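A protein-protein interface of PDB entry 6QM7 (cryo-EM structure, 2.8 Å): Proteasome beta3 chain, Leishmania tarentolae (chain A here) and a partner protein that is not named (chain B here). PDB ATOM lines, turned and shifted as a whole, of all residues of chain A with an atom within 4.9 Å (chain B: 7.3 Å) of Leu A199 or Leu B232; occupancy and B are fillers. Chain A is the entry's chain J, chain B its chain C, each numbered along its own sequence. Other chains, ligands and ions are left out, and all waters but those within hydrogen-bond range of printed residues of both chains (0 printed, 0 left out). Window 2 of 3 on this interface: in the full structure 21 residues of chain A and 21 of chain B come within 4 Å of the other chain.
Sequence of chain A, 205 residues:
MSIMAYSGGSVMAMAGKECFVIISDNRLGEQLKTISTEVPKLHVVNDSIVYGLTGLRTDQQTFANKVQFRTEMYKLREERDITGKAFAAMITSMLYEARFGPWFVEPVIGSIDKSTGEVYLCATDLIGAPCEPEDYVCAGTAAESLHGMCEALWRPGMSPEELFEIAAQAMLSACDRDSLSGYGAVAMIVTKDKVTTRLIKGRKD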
ATOM      1  N   ASN A  26      -2.260  21.973 -23.086  1.00  0.00           N
ATOM      2  CA  ASN A  26      -3.356  21.184 -22.477  1.00  0.00           C
ATOM      3  C   ASN A  26      -4.229  20.502 -23.534  1.00  0.00           C
ATOM      4  O   ASN A  26      -5.143  19.773 -23.142  1.00  0.00           O
ATOM      5  CB  ASN A  26      -4.263  22.094 -21.652  1.00  0.00           C
ATOM      6  CG  ASN A  26      -3.651  22.543 -20.351  1.00  0.00           C
ATOM      7  OD1 ASN A  26      -3.553  23.741 -20.088  1.00  0.00           O
ATOM      8  ND2 ASN A  26      -3.297  21.574 -19.523  1.00  0.00           N
ATOM      9  N   PRO A  40      -2.759  17.853 -19.798  1.00  0.00           N
ATOM     10  CA  PRO A  40      -1.358  18.242 -19.766  1.00  0.00           C
ATOM     11  C   PRO A  40      -0.543  16.981 -20.071  1.00  0.00           C
ATOM     12  O   PRO A  40      -1.028  15.886 -19.832  1.00  0.00           O
ATOM     13  CB  PRO A  40      -1.107  18.769 -18.350  1.00  0.00           C
ATOM     14  CG  PRO A  40      -2.462  18.728 -17.658  1.00  0.00           C
ATOM     15  CD  PRO A  40      -3.352  17.805 -18.462  1.00  0.00           C
ATOM     16  N   ALA A 185      -1.676  26.187 -20.604  1.00  0.00           N
ATOM     17  CA  ALA A 185      -0.500  25.354 -20.340  1.00  0.00           C
ATOM     18  C   ALA A 185      -0.437  25.017 -18.863  1.00  0.00           C
ATOM     19  O   ALA A 185      -0.851  25.841 -18.065  1.00  0.00           O
ATOM     20  CB  ALA A 185       0.715  26.102 -20.795  1.00  0.00           C
ATOM     21  N   VAL A 186       0.037  23.824 -18.537  1.00  0.00           N
ATOM     22  CA  VAL A 186       0.509  23.499 -17.168  1.00  0.00           C
ATOM     23  C   VAL A 186       2.027  23.573 -17.207  1.00  0.00           C
ATOM     24  O   VAL A 186       2.620  22.937 -18.078  1.00  0.00           O
ATOM     25  CB  VAL A 186       0.015  22.123 -16.708  1.00  0.00           C
ATOM     26  CG1 VAL A 186       0.729  21.672 -15.453  1.00  0.00           C
ATOM     27  CG2 VAL A 186      -1.489  22.134 -16.503  1.00  0.00           C
ATOM     28  N   THR A 197       3.738  24.070  -9.297  1.00  0.00           N
ATOM     29  CA  THR A 197       2.964  23.709 -10.510  1.00  0.00           C
ATOM     30  C   THR A 197       1.983  24.840 -10.777  1.00  0.00           C
ATOM     31  O   THR A 197       1.337  25.255  -9.829  1.00  0.00           O
ATOM     32  CB  THR A 197       2.232  22.370 -10.346  1.00  0.00           C
ATOM     33  OG1 THR A 197       3.149  21.392  -9.841  1.00  0.00           O
ATOM     34  CG2 THR A 197       1.633  21.877 -11.650  1.00  0.00           C
ATOM     35  N   ARG A 198       1.881  25.306 -12.011  1.00  0.00           N
ATOM     36  CA  ARG A 198       0.996  26.437 -12.374  1.00  0.00           C
ATOM     37  C   ARG A 198       0.223  26.111 -13.640  1.00  0.00           C
ATOM     38  O   ARG A 198       0.858  25.789 -14.651  1.00  0.00           O
ATOM     39  CB  ARG A 198       1.806  27.702 -12.621  1.00  0.00           C
ATOM     40  CG  ARG A 198       2.546  28.176 -11.387  1.00  0.00           C
ATOM     41  CD  ARG A 198       2.969  29.614 -11.535  1.00  0.00           C
ATOM     42  NE  ARG A 198       3.487  30.063 -10.260  1.00  0.00           N
ATOM     43  CZ  ARG A 198       4.645  30.674 -10.060  1.00  0.00           C
ATOM     44  NH1 ARG A 198       5.445  30.978 -11.071  1.00  0.00           N
ATOM     45  NH2 ARG A 198       4.985  31.007  -8.826  1.00  0.00           N
ATOM     46  N   LEU A 199      -1.099  26.193 -13.550  1.00  0.00           N
ATOM     47  CA  LEU A 199      -2.006  26.247 -14.719  1.00  0.00           C
ATOM     48  C   LEU A 199      -2.014  27.689 -15.238  1.00  0.00           C
ATOM     49  O   LEU A 199      -2.274  28.598 -14.462  1.00  0.00           O
ATOM     50  CB  LEU A 199      -3.384  25.762 -14.262  1.00  0.00           C
ATOM     51  CG  LEU A 199      -4.467  25.722 -15.330  1.00  0.00           C
ATOM     52  CD1 LEU A 199      -4.045  24.892 -16.541  1.00  0.00           C
ATOM     53  CD2 LEU A 199      -5.754  25.192 -14.732  1.00  0.00           C
ATOM     54  N   ILE A 200      -1.686  27.879 -16.506  1.00  0.00           N
ATOM     55  CA  ILE A 200      -1.497  29.202 -17.166  1.00  0.00           C
ATOM     56  C   ILE A 200      -2.711  29.465 -18.054  1.00  0.00           C
ATOM     57  O   ILE A 200      -3.052  28.597 -18.865  1.00  0.00           O
ATOM     58  CB  ILE A 200      -0.192  29.183 -17.979  1.00  0.00           C
ATOM     59  CG1 ILE A 200       1.027  29.019 -17.077  1.00  0.00           C
ATOM     60  CG2 ILE A 200      -0.052  30.403 -18.864  1.00  0.00           C
ATOM     61  CD1 ILE A 200       2.186  28.353 -17.782  1.00  0.00           C
ATOM     62  N   LYS A 201      -3.338  30.625 -17.886  1.00  0.00           N
ATOM     63  CA  LYS A 201      -4.486  31.069 -18.712  1.00  0.00           C
ATOM     64  C   LYS A 201      -3.935  31.357 -20.108  1.00  0.00           C
ATOM     65  O   LYS A 201      -2.993  32.172 -20.219  1.00  0.00           O
ATOM     66  CB  LYS A 201      -5.206  32.262 -18.065  1.00  0.00           C
ATOM     67  CG  LYS A 201      -5.774  33.313 -19.012  1.00  0.00           C
ATOM     68  CD  LYS A 201      -7.044  33.995 -18.509  1.00  0.00           C
ATOM     69  CE  LYS A 201      -7.510  35.122 -19.416  1.00  0.00           C
ATOM     70  NZ  LYS A 201      -7.557  34.724 -20.848  1.00  0.00           N
ATOM     71  N   ILE B 229       0.189  15.151  -4.420  1.00  0.00           N
ATOM     72  CA  ILE B 229      -1.078  14.959  -5.188  1.00  0.00           C
ATOM     73  C   ILE B 229      -0.747  15.186  -6.673  1.00  0.00           C
ATOM     74  O   ILE B 229      -0.912  14.230  -7.462  1.00  0.00           O
ATOM     75  CB  ILE B 229      -2.211  15.892  -4.680  1.00  0.00           C
ATOM     76  CG1 ILE B 229      -2.402  15.865  -3.157  1.00  0.00           C
ATOM     77  CG2 ILE B 229      -3.523  15.593  -5.392  1.00  0.00           C
ATOM     78  CD1 ILE B 229      -2.978  14.576  -2.609  1.00  0.00           C
ATOM     79  N   ASP B 230      -0.258  16.391  -7.014  1.00  0.00           N
ATOM     80  CA  ASP B 230       0.035  16.888  -8.393  1.00  0.00           C
ATOM     81  C   ASP B 230      -1.267  16.872  -9.208  1.00  0.00           C
ATOM     82  O   ASP B 230      -1.263  16.316 -10.327  1.00  0.00           O
ATOM     83  CB  ASP B 230       1.176  16.104  -9.064  1.00  0.00           C
ATOM     84  CG  ASP B 230       2.566  16.335  -8.478  1.00  0.00           C
ATOM     85  OD1 ASP B 230       2.855  17.479  -8.063  1.00  0.00           O
ATOM     86  OD2 ASP B 230       3.360  15.371  -8.453  1.00  0.00           O
ATOM     87  N   GLN B 231      -2.330  17.478  -8.663  1.00  0.00           N
ATOM     88  CA  GLN B 231      -3.720  17.420  -9.200  1.00  0.00           C
ATOM     89  C   GLN B 231      -3.795  18.109 -10.572  1.00  0.00           C
ATOM     90  O   GLN B 231      -4.597  17.646 -11.400  1.00  0.00           O
ATOM     91  CB  GLN B 231      -4.718  18.054  -8.222  1.00  0.00           C
ATOM     92  CG  GLN B 231      -6.193  17.913  -8.612  1.00  0.00           C
ATOM     93  CD  GLN B 231      -6.709  16.495  -8.552  1.00  0.00           C
ATOM     94  OE1 GLN B 231      -6.893  15.929  -7.477  1.00  0.00           O
ATOM     95  NE2 GLN B 231      -6.956  15.909  -9.712  1.00  0.00           N
ATOM     96  N   LEU B 232      -3.007  19.161 -10.812  1.00  0.00           N
ATOM     97  CA  LEU B 232      -3.068  19.944 -12.073  1.00  0.00           C
ATOM     98  C   LEU B 232      -2.498  19.147 -13.250  1.00  0.00           C
ATOM     99  O   LEU B 232      -2.774  19.558 -14.395  1.00  0.00           O
ATOM    100  CB  LEU B 232      -2.291  21.251 -11.915  1.00  0.00           C
ATOM    101  CG  LEU B 232      -2.821  22.221 -10.865  1.00  0.00           C
ATOM    102  CD1 LEU B 232      -2.008  23.502 -10.877  1.00  0.00           C
ATOM    103  CD2 LEU B 232      -4.292  22.524 -11.092  1.00  0.00           C
ATOM    104  N   LEU B 233      -1.727  18.081 -13.005  1.00  0.00           N
ATOM    105  CA  LEU B 233      -1.101  17.262 -14.081  1.00  0.00           C
ATOM    106  C   LEU B 233      -2.095  16.246 -14.659  1.00  0.00           C
ATOM    107  O   LEU B 233      -1.949  15.905 -15.858  1.00  0.00           O
ATOM    108  CB  LEU B 233       0.136  16.550 -13.541  1.00  0.00           C
ATOM    109  CG  LEU B 233       1.325  17.437 -13.188  1.00  0.00           C
ATOM    110  CD1 LEU B 233       2.571  16.584 -13.035  1.00  0.00           C
ATOM    111  CD2 LEU B 233       1.561  18.516 -14.228  1.00  0.00           C
ATOM    112  N   ASP B 234      -3.032  15.758 -13.844  1.00  0.00           N
ATOM    113  CA  ASP B 234      -4.203  14.964 -14.308  1.00  0.00           C
ATOM    114  C   ASP B 234      -5.438  15.464 -13.555  1.00  0.00           C
ATOM    115  O   ASP B 234      -5.739  14.990 -12.461  1.00  0.00           O
ATOM    116  CB  ASP B 234      -3.921  13.464 -14.192  1.00  0.00           C
ATOM    117  CG  ASP B 234      -4.651  12.619 -15.230  1.00  0.00           C
ATOM    118  OD1 ASP B 234      -5.802  12.978 -15.597  1.00  0.00           O
ATOM    119  OD2 ASP B 234      -4.062  11.606 -15.675  1.00  0.00           O
ATOM    120  N   PRO B 235      -6.151  16.480 -14.099  1.00  0.00           N
ATOM    121  CA  PRO B 235      -7.325  17.058 -13.441  1.00  0.00           C
ATOM    122  C   PRO B 235      -8.449  16.088 -13.055  1.00  0.00           C
ATOM    123  O   PRO B 235      -9.136  16.353 -12.092  1.00  0.00           O
ATOM    124  CB  PRO B 235      -7.894  18.029 -14.490  1.00  0.00           C
ATOM    125  CG  PRO B 235      -6.698  18.408 -15.335  1.00  0.00           C
ATOM    126  CD  PRO B 235      -5.823  17.174 -15.353  1.00  0.00           C
ATOM    127  N   HIS B 239      -7.233  11.396  -6.351  1.00  0.00           N
ATOM    128  CA  HIS B 239      -6.170  11.034  -5.385  1.00  0.00           C
ATOM    129  C   HIS B 239      -6.833  10.874  -4.025  1.00  0.00           C
ATOM    130  O   HIS B 239      -7.446  11.818  -3.536  1.00  0.00           O
ATOM    131  CB  HIS B 239      -5.050  12.081  -5.412  1.00  0.00           C
ATOM    132  CG  HIS B 239      -4.435  12.251  -6.762  1.00  0.00           C
ATOM    133  ND1 HIS B 239      -3.555  11.325  -7.292  1.00  0.00           N
ATOM    134  CD2 HIS B 239      -4.574  13.227  -7.691  1.00  0.00           C
ATOM    135  CE1 HIS B 239      -3.171  11.725  -8.490  1.00  0.00           C
ATOM    136  NE2 HIS B 239      -3.788  12.890  -8.760  1.00  0.00           N
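Among the printed residues, pairs that only touch across the chains: Pro A40 with Leu B232 (3.4 Å), Pro A40 with Leu B233 (3.4 Å), Val A186 with Leu B233 (3.5 Å), Val A186 with Leu B232 (3.6 Å), Leu A199 with Leu B232 (3.9 Å) and Thr A197 with Leu B232 (3.9 Å).
Of chain B, only Leu B232 comes within 4 Å of Leu A199. Leu B232 touches just these residues of chain A: Pro A40, Val A186, Thr A197 and Leu A199. Of the printed residues of chain B, Pro A40 touches Leu B232 and Leu B233. Of the printed residues of chain B, Val A186 touches Leu B232 (3.6 Å) and Leu B233 (3.5 Å). Printed residues of chain A within 4 Å of Leu B233: Pro A40 and Val A186. Ala A185 touches none of the printed residues of chain B.
Of the 9 printed residues of chain A, 4 touch a printed residue of chain B. Printed residues of chain A that touch a printed residue of chain B: Pro A40, Val A186, Thr A197 and Leu A199. Along chain A the printed residues that touch a printed residue of chain B span positions 40 to 199. Printed residues of chain B that touch a printed residue of chain A: Leu B232 and Leu B233. Hydrophobic or aromatic side chains of chain B that line the printed part of chain A: Leu B232 and Leu B233. Among the printed residues, no Asp or Glu carboxylate lies within 4 Å of a Lys or Arg side-chain nitrogen of the other chain.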
